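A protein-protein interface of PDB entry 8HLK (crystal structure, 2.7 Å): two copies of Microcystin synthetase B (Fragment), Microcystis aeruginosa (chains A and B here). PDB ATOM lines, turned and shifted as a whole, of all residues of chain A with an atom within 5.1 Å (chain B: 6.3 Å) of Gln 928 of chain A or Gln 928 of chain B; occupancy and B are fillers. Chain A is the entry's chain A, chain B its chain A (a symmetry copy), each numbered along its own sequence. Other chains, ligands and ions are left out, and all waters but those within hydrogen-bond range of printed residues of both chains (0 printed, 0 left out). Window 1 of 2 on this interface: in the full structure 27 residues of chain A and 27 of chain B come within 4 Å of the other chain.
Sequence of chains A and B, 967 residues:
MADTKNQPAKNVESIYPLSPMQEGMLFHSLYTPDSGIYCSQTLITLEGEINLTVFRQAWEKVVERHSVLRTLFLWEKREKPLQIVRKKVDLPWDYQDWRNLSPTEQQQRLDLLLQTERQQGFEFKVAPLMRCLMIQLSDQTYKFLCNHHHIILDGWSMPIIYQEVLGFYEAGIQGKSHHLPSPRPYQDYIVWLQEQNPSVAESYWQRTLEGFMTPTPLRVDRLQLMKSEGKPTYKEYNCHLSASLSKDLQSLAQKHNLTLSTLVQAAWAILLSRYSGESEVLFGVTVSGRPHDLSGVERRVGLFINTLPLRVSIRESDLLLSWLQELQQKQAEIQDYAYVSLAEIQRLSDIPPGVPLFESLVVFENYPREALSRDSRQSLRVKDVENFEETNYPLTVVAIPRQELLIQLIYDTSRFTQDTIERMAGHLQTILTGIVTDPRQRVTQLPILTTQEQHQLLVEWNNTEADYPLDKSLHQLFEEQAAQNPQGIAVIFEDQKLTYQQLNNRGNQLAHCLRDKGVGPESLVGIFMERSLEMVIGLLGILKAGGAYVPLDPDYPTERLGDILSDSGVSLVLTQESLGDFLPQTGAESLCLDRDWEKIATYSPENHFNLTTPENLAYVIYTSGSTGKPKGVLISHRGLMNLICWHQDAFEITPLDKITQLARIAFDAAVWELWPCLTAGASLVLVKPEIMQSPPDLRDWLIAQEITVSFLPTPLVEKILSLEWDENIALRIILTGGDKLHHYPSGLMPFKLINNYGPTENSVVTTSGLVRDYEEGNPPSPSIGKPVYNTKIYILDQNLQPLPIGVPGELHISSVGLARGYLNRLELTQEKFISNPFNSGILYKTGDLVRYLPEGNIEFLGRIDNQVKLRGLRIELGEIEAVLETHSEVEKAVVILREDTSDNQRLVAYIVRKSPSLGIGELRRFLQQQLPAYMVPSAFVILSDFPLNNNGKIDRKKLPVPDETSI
Arg 925 of chain B touches its own counterpart, Arg 925 of chain A.
Arg 925 of chain A touches Gln 928 of chain B, and with the chains exchanged Gln 928 of chain A touches Arg 925 of chain B.
Arg 925 of chain A touches Gln 929 of chain B, and with the chains exchanged Gln 929 of chain A touches Arg 925 of chain B.
Gln 928 of chain B touches its own counterpart, Gln 928 of chain A.
Of the 6 pairs that touch across the chains among the printed residues, 6 have their exchanged pair printed and touching as well.
OE1 of Gln 928 of chain B lies within hydrogen-bond range of NE2 of Gln 928 of chain A (3.2 Å).
Among the printed residues, pairs that only touch across the chains: Arg 925 of chain A with Arg 925 of chain B, Arg 925 of chain A with Gln 928 of chain B, Arg 925 of chain A with Gln 929 of chain B, Gln 928 of chain A with Arg 925 of chain B and Gln 929 of chain A with Arg 925 of chain B.
Arg 924 of chain A touches none of the printed residues of chain B.
Printed residues of chain B within 4 Å of Arg 925 of chain A: Arg 925, Gln 928 and Gln 929.
Of chain B, only Arg 925 (3.5 Å) and Gln 928 (3.2 Å) come within 4 Å of Gln 928 of chain A.
Of the printed residues of chain B, Gln 929 of chain A touches Arg 925.
Leu 931 of chain A touches none of the printed residues of chain B.
Of the printed residues of chain A, Arg 925 of chain B touches Arg 925 (3.7 Å), Gln 928 (3.5 Å) and Gln 929 (3.7 Å).
Of the printed residues of chain A, Gln 928 of chain B touches Arg 925 (3.5 Å) and Gln 928 (3.2 Å).
The nearest residue of chain B that does not touch Gln 928 of chain A is Arg 924 of chain B (4.5 Å).
The nearest residue of chain A that does not touch Gln 928 of chain B is Arg 924 of chain A (4.5 Å).
Of the 10 printed residues of chain A, 3 touch a printed residue of chain B.
Printed residues of chain B that touch a printed residue of chain A: Arg 925, Gln 928 and Gln 929.
Among the printed residues, 6 pairs touch across the chains.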
ATOM      1  N   ARG A 924       3.304 -16.751 -22.494  1.00  0.00           N
ATOM      2  CA  ARG A 924       2.932 -17.447 -23.723  1.00  0.00           C
ATOM      3  C   ARG A 924       3.752 -16.931 -24.908  1.00  0.00           C
ATOM      4  O   ARG A 924       4.312 -17.709 -25.671  1.00  0.00           O
ATOM      5  CB  ARG A 924       1.431 -17.330 -24.022  1.00  0.00           C
ATOM      6  CG  ARG A 924       0.909 -18.368 -25.015  1.00  0.00           C
ATOM      7  CD  ARG A 924      -0.605 -18.503 -25.067  1.00  0.00           C
ATOM      8  NE  ARG A 924      -1.178 -18.997 -23.807  1.00  0.00           N
ATOM      9  CZ  ARG A 924      -1.980 -18.307 -22.987  1.00  0.00           C
ATOM     10  NH1 ARG A 924      -2.320 -17.059 -23.265  1.00  0.00           N
ATOM     11  NH2 ARG A 924      -2.441 -18.872 -21.881  1.00  0.00           N
ATOM     12  N   ARG A 925       3.852 -15.616 -25.057  1.00  0.00           N
ATOM     13  CA  ARG A 925       4.628 -15.039 -26.143  1.00  0.00           C
ATOM     14  C   ARG A 925       6.121 -15.322 -25.964  1.00  0.00           C
ATOM     15  O   ARG A 925       6.851 -15.439 -26.943  1.00  0.00           O
ATOM     16  CB  ARG A 925       4.358 -13.535 -26.202  1.00  0.00           C
ATOM     17  CG  ARG A 925       2.909 -13.201 -26.523  1.00  0.00           C
ATOM     18  CD  ARG A 925       2.561 -11.748 -26.285  1.00  0.00           C
ATOM     19  NE  ARG A 925       1.155 -11.701 -25.931  1.00  0.00           N
ATOM     20  CZ  ARG A 925       0.698 -11.378 -24.726  1.00  0.00           C
ATOM     21  NH1 ARG A 925       1.506 -10.820 -23.835  1.00  0.00           N
ATOM     22  NH2 ARG A 925      -0.577 -11.583 -24.430  1.00  0.00           N
ATOM     23  N   PHE A 926       6.587 -15.389 -24.712  1.00  0.00           N
ATOM     24  CA  PHE A 926       7.982 -15.693 -24.448  1.00  0.00           C
ATOM     25  C   PHE A 926       8.331 -17.077 -24.984  1.00  0.00           C
ATOM     26  O   PHE A 926       9.404 -17.265 -25.531  1.00  0.00           O
ATOM     27  CB  PHE A 926       8.309 -15.625 -22.959  1.00  0.00           C
ATOM     28  CG  PHE A 926       9.709 -16.069 -22.647  1.00  0.00           C
ATOM     29  CD1 PHE A 926      10.737 -15.145 -22.577  1.00  0.00           C
ATOM     30  CD2 PHE A 926      10.002 -17.406 -22.428  1.00  0.00           C
ATOM     31  CE1 PHE A 926      12.035 -15.540 -22.285  1.00  0.00           C
ATOM     32  CE2 PHE A 926      11.302 -17.800 -22.142  1.00  0.00           C
ATOM     33  CZ  PHE A 926      12.318 -16.869 -22.076  1.00  0.00           C
ATOM     34  N   LEU A 927       7.421 -18.038 -24.837  1.00  0.00           N
ATOM     35  CA  LEU A 927       7.691 -19.402 -25.263  1.00  0.00           C
ATOM     36  C   LEU A 927       7.457 -19.597 -26.768  1.00  0.00           C
ATOM     37  O   LEU A 927       8.041 -20.515 -27.340  1.00  0.00           O
ATOM     38  CB  LEU A 927       6.842 -20.374 -24.435  1.00  0.00           C
ATOM     39  CG  LEU A 927       7.187 -21.855 -24.598  1.00  0.00           C
ATOM     40  CD1 LEU A 927       8.564 -22.157 -24.017  1.00  0.00           C
ATOM     41  CD2 LEU A 927       6.121 -22.743 -23.968  1.00  0.00           C
ATOM     42  N   GLN A 928       6.629 -18.764 -27.432  1.00  0.00           N
ATOM     43  CA  GLN A 928       6.476 -18.876 -28.888  1.00  0.00           C
ATOM     44  C   GLN A 928       7.588 -18.095 -29.595  1.00  0.00           C
ATOM     45  O   GLN A 928       7.817 -18.332 -30.775  1.00  0.00           O
ATOM     46  CB  GLN A 928       5.067 -18.530 -29.415  1.00  0.00           C
ATOM     47  CG  GLN A 928       4.484 -17.184 -28.985  1.00  0.00           C
ATOM     48  CD  GLN A 928       3.043 -16.987 -29.415  1.00  0.00           C
ATOM     49  OE1 GLN A 928       2.139 -17.705 -28.989  1.00  0.00           O
ATOM     50  NE2 GLN A 928       2.806 -15.992 -30.259  1.00  0.00           N
ATOM     51  N   GLN A 929       8.278 -17.207 -28.857  1.00  0.00           N
ATOM     52  CA  GLN A 929       9.538 -16.603 -29.272  1.00  0.00           C
ATOM     53  C   GLN A 929      10.689 -17.620 -29.287  1.00  0.00           C
ATOM     54  O   GLN A 929      11.540 -17.535 -30.169  1.00  0.00           O
ATOM     55  CB  GLN A 929       9.932 -15.449 -28.341  1.00  0.00           C
ATOM     56  CG  GLN A 929       9.359 -14.095 -28.734  1.00  0.00           C
ATOM     57  CD  GLN A 929       9.847 -12.978 -27.841  1.00  0.00           C
ATOM     58  OE1 GLN A 929      10.494 -13.198 -26.814  1.00  0.00           O
ATOM     59  NE2 GLN A 929       9.535 -11.753 -28.236  1.00  0.00           N
ATOM     60  N   GLN A 930      10.763 -18.523 -28.289  1.00  0.00           N
ATOM     61  CA  GLN A 930      11.944 -19.346 -28.064  1.00  0.00           C
ATOM     62  C   GLN A 930      11.799 -20.641 -28.844  1.00  0.00           C
ATOM     63  O   GLN A 930      12.612 -20.951 -29.705  1.00  0.00           O
ATOM     64  CB  GLN A 930      12.156 -19.680 -26.587  1.00  0.00           C
ATOM     65  CG  GLN A 930      12.362 -18.472 -25.688  1.00  0.00           C
ATOM     66  CD  GLN A 930      13.567 -17.659 -26.074  1.00  0.00           C
ATOM     67  OE1 GLN A 930      13.451 -16.521 -26.518  1.00  0.00           O
ATOM     68  NE2 GLN A 930      14.734 -18.250 -25.917  1.00  0.00           N
ATOM     69  N   LEU A 931      10.765 -21.412 -28.528  1.00  0.00           N
ATOM     70  CA  LEU A 931      10.396 -22.510 -29.397  1.00  0.00           C
ATOM     71  C   LEU A 931       9.494 -21.911 -30.468  1.00  0.00           C
ATOM     72  O   LEU A 931       9.280 -20.704 -30.455  1.00  0.00           O
ATOM     73  CB  LEU A 931       9.760 -23.629 -28.554  1.00  0.00           C
ATOM     74  CG  LEU A 931      10.745 -24.722 -28.114  1.00  0.00           C
ATOM     75  CD1 LEU A 931      11.781 -24.178 -27.142  1.00  0.00           C
ATOM     76  CD2 LEU A 931      10.036 -25.922 -27.511  1.00  0.00           C
ATOM     77  N   PRO A 932       9.042 -22.665 -31.490  1.00  0.00           N
ATOM     78  CA  PRO A 932       7.878 -22.254 -32.276  1.00  0.00           C
ATOM     79  C   PRO A 932       6.584 -22.682 -31.567  1.00  0.00           C
ATOM     80  O   PRO A 932       6.589 -22.897 -30.361  1.00  0.00           O
ATOM     81  CB  PRO A 932       8.181 -22.926 -33.630  1.00  0.00           C
ATOM     82  CG  PRO A 932       8.890 -24.216 -33.266  1.00  0.00           C
ATOM     83  CD  PRO A 932       9.672 -23.891 -32.008  1.00  0.00           C
ATOM     84  N   VAL A 936       4.338 -25.094 -27.697  1.00  0.00           N
ATOM     85  CA  VAL A 936       3.819 -24.144 -26.733  1.00  0.00           C
ATOM     86  C   VAL A 936       2.479 -24.709 -26.268  1.00  0.00           C
ATOM     87  O   VAL A 936       1.672 -25.149 -27.089  1.00  0.00           O
ATOM     88  CB  VAL A 936       3.696 -22.722 -27.326  1.00  0.00           C
ATOM     89  CG1 VAL A 936       2.942 -21.764 -26.414  1.00  0.00           C
ATOM     90  CG2 VAL A 936       5.057 -22.141 -27.672  1.00  0.00           C
ATOM     91  N   GLY B 921       5.768 -12.961 -36.792  1.00  0.00           N
ATOM     92  CA  GLY B 921       5.743 -13.279 -35.373  1.00  0.00           C
ATOM     93  C   GLY B 921       5.234 -12.101 -34.539  1.00  0.00           C
ATOM     94  O   GLY B 921       4.294 -12.266 -33.766  1.00  0.00           O
ATOM     95  N   LEU B 923       3.646  -9.441 -35.407  1.00  0.00           N
ATOM     96  CA  LEU B 923       2.246  -9.294 -35.754  1.00  0.00           C
ATOM     97  C   LEU B 923       1.426 -10.285 -34.928  1.00  0.00           C
ATOM     98  O   LEU B 923       0.469  -9.884 -34.277  1.00  0.00           O
ATOM     99  CB  LEU B 923       2.114  -9.534 -37.265  1.00  0.00           C
ATOM    100  CG  LEU B 923       0.833  -9.047 -37.947  1.00  0.00           C
ATOM    101  CD1 LEU B 923       0.759  -7.525 -37.978  1.00  0.00           C
ATOM    102  CD2 LEU B 923       0.730  -9.602 -39.362  1.00  0.00           C
ATOM    103  N   ARG B 924       1.822 -11.566 -34.908  1.00  0.00           N
ATOM    104  CA  ARG B 924       1.029 -12.611 -34.267  1.00  0.00           C
ATOM    105  C   ARG B 924       0.778 -12.276 -32.795  1.00  0.00           C
ATOM    106  O   ARG B 924      -0.348 -12.343 -32.318  1.00  0.00           O
ATOM    107  CB  ARG B 924       1.681 -13.994 -34.396  1.00  0.00           C
ATOM    108  CG  ARG B 924       0.726 -15.161 -34.148  1.00  0.00           C
ATOM    109  CD  ARG B 924       1.240 -16.519 -34.599  1.00  0.00           C
ATOM    110  NE  ARG B 924       1.425 -16.604 -36.055  1.00  0.00           N
ATOM    111  CZ  ARG B 924       2.595 -16.744 -36.689  1.00  0.00           C
ATOM    112  NH1 ARG B 924       3.730 -16.806 -36.012  1.00  0.00           N
ATOM    113  NH2 ARG B 924       2.628 -16.819 -38.011  1.00  0.00           N
ATOM    114  N   ARG B 925       1.820 -11.886 -32.070  1.00  0.00           N
ATOM    115  CA  ARG B 925       1.669 -11.529 -30.669  1.00  0.00           C
ATOM    116  C   ARG B 925       0.843 -10.251 -30.512  1.00  0.00           C
ATOM    117  O   ARG B 925       0.148 -10.081 -29.515  1.00  0.00           O
ATOM    118  CB  ARG B 925       3.057 -11.365 -30.046  1.00  0.00           C
ATOM    119  CG  ARG B 925       3.867 -12.652 -30.047  1.00  0.00           C
ATOM    120  CD  ARG B 925       5.329 -12.441 -29.723  1.00  0.00           C
ATOM    121  NE  ARG B 925       6.071 -13.480 -30.412  1.00  0.00           N
ATOM    122  CZ  ARG B 925       6.891 -13.261 -31.434  1.00  0.00           C
ATOM    123  NH1 ARG B 925       7.284 -12.027 -31.720  1.00  0.00           N
ATOM    124  NH2 ARG B 925       7.345 -14.283 -32.144  1.00  0.00           N
ATOM    125  N   PHE B 926       0.949  -9.329 -31.474  1.00  0.00           N
ATOM    126  CA  PHE B 926       0.171  -8.104 -31.427  1.00  0.00           C
ATOM    127  C   PHE B 926      -1.319  -8.424 -31.467  1.00  0.00           C
ATOM    128  O   PHE B 926      -2.096  -7.793 -30.770  1.00  0.00           O
ATOM    129  CB  PHE B 926       0.521  -7.161 -32.575  1.00  0.00           C
ATOM    130  CG  PHE B 926      -0.365  -5.951 -32.628  1.00  0.00           C
ATOM    131  CD1 PHE B 926       0.010  -4.780 -31.991  1.00  0.00           C
ATOM    132  CD2 PHE B 926      -1.572  -5.979 -33.308  1.00  0.00           C
ATOM    133  CE1 PHE B 926      -0.797  -3.652 -32.036  1.00  0.00           C
ATOM    134  CE2 PHE B 926      -2.381  -4.851 -33.346  1.00  0.00           C
ATOM    135  CZ  PHE B 926      -1.997  -3.691 -32.706  1.00  0.00           C
ATOM    136  N   LEU B 927      -1.713  -9.410 -32.272  1.00  0.00           N
ATOM    137  CA  LEU B 927      -3.120  -9.744 -32.419  1.00  0.00           C
ATOM    138  C   LEU B 927      -3.623 -10.650 -31.286  1.00  0.00           C
ATOM    139  O   LEU B 927      -4.824 -10.653 -31.025  1.00  0.00           O
ATOM    140  CB  LEU B 927      -3.352 -10.386 -33.793  1.00  0.00           C
ATOM    141  CG  LEU B 927      -4.816 -10.575 -34.194  1.00  0.00           C
ATOM    142  CD1 LEU B 927      -5.493  -9.228 -34.421  1.00  0.00           C
ATOM    143  CD2 LEU B 927      -4.941 -11.465 -35.424  1.00  0.00           C
ATOM    144  N   GLN B 928      -2.750 -11.413 -30.598  1.00  0.00           N
ATOM    145  CA  GLN B 928      -3.201 -12.205 -29.448  1.00  0.00           C
ATOM    146  C   GLN B 928      -3.209 -11.339 -28.185  1.00  0.00           C
ATOM    147  O   GLN B 928      -3.853 -11.719 -27.212  1.00  0.00           O
ATOM    148  CB  GLN B 928      -2.458 -13.545 -29.256  1.00  0.00           C
ATOM    149  CG  GLN B 928      -0.931 -13.481 -29.210  1.00  0.00           C
ATOM    150  CD  GLN B 928      -0.272 -14.847 -29.175  1.00  0.00           C
ATOM    151  OE1 GLN B 928      -0.380 -15.639 -30.111  1.00  0.00           O
ATOM    152  NE2 GLN B 928       0.437 -15.136 -28.093  1.00  0.00           N
ATOM    153  N   GLN B 929      -2.529 -10.180 -28.231  1.00  0.00           N
ATOM    154  CA  GLN B 929      -2.668  -9.111 -27.251  1.00  0.00           C
ATOM    155  C   GLN B 929      -4.034  -8.414 -27.344  1.00  0.00           C
ATOM    156  O   GLN B 929      -4.579  -8.043 -26.308  1.00  0.00           O
ATOM    157  CB  GLN B 929      -1.577  -8.047 -27.433  1.00  0.00           C
ATOM    158  CG  GLN B 929      -0.286  -8.329 -26.678  1.00  0.00           C
ATOM    159  CD  GLN B 929       0.723  -7.212 -26.816  1.00  0.00           C
ATOM    160  OE1 GLN B 929       0.556  -6.275 -27.601  1.00  0.00           O
ATOM    161  NE2 GLN B 929       1.790  -7.308 -26.040  1.00  0.00           N
ATOM    162  N   GLN B 930      -4.551  -8.173 -28.566  1.00  0.00           N
ATOM    163  CA  GLN B 930      -5.694  -7.293 -28.771  1.00  0.00           C
ATOM    164  C   GLN B 930      -6.969  -8.117 -28.707  1.00  0.00           C
ATOM    165  O   GLN B 930      -7.830  -7.879 -27.871  1.00  0.00           O
ATOM    166  CB  GLN B 930      -5.644  -6.566 -30.116  1.00  0.00           C
ATOM    167  CG  GLN B 930      -4.435  -5.663 -30.302  1.00  0.00           C
ATOM    168  CD  GLN B 930      -4.363  -4.570 -29.272  1.00  0.00           C
ATOM    169  OE1 GLN B 930      -3.467  -4.542 -28.434  1.00  0.00           O
ATOM    170  NE2 GLN B 930      -5.321  -3.667 -29.324  1.00  0.00           N
ATOM    171  N   LEU B 931      -7.098  -9.082 -29.609  1.00  0.00           N
ATOM    172  CA  LEU B 931      -8.133 -10.082 -29.449  1.00  0.00           C
ATOM    173  C   LEU B 931      -7.545 -11.150 -28.536  1.00  0.00           C
ATOM    174  O   LEU B 931      -6.416 -10.990 -28.088  1.00  0.00           O
ATOM    175  CB  LEU B 931      -8.578 -10.575 -30.837  1.00  0.00           C
ATOM    176  CG  LEU B 931      -9.807  -9.847 -31.400  1.00  0.00           C
ATOM    177  CD1 LEU B 931      -9.500  -8.386 -31.695  1.00  0.00           C
ATOM    178  CD2 LEU B 931     -10.359 -10.530 -32.639  1.00  0.00           C
ATOM    179  N   PRO B 932      -8.296 -12.190 -28.121  1.00  0.00           N
ATOM    180  CA  PRO B 932      -7.675 -13.413 -27.608  1.00  0.00           C
ATOM    181  C   PRO B 932      -7.285 -14.335 -28.774  1.00  0.00           C
ATOM    182  O   PRO B 932      -7.123 -13.870 -29.895  1.00  0.00           O
ATOM    183  CB  PRO B 932      -8.772 -13.927 -26.655  1.00  0.00           C
ATOM    184  CG  PRO B 932     -10.075 -13.522 -27.319  1.00  0.00           C
ATOM    185  CD  PRO B 932      -9.764 -12.217 -28.026  1.00  0.00           C
ATOM    186  N   ALA B 933      -7.083 -15.633 -28.505  1.00  0.00           N
ATOM    187  CA  ALA B 933      -6.894 -16.637 -29.549  1.00  0.00           C
ATOM    188  C   ALA B 933      -8.264 -17.090 -30.066  1.00  0.00           C
ATOM    189  O   ALA B 933      -9.298 -16.612 -29.587  1.00  0.00           O
ATOM    190  CB  ALA B 933      -6.230 -17.873 -28.972  1.00  0.00           C
ATOM    191  N   VAL B 936      -7.276 -15.262 -33.771  1.00  0.00           N
ATOM    192  CA  VAL B 936      -5.961 -15.025 -34.335  1.00  0.00           C
ATOM    193  C   VAL B 936      -5.741 -16.131 -35.364  1.00  0.00           C
ATOM    194  O   VAL B 936      -6.012 -17.301 -35.087  1.00  0.00           O
ATOM    195  CB  VAL B 936      -4.862 -14.990 -33.249  1.00  0.00           C
ATOM    196  CG1 VAL B 936      -3.456 -14.973 -33.832  1.00  0.00           C
ATOM    197  CG2 VAL B 936      -5.043 -13.809 -32.309  1.00  0.00           C
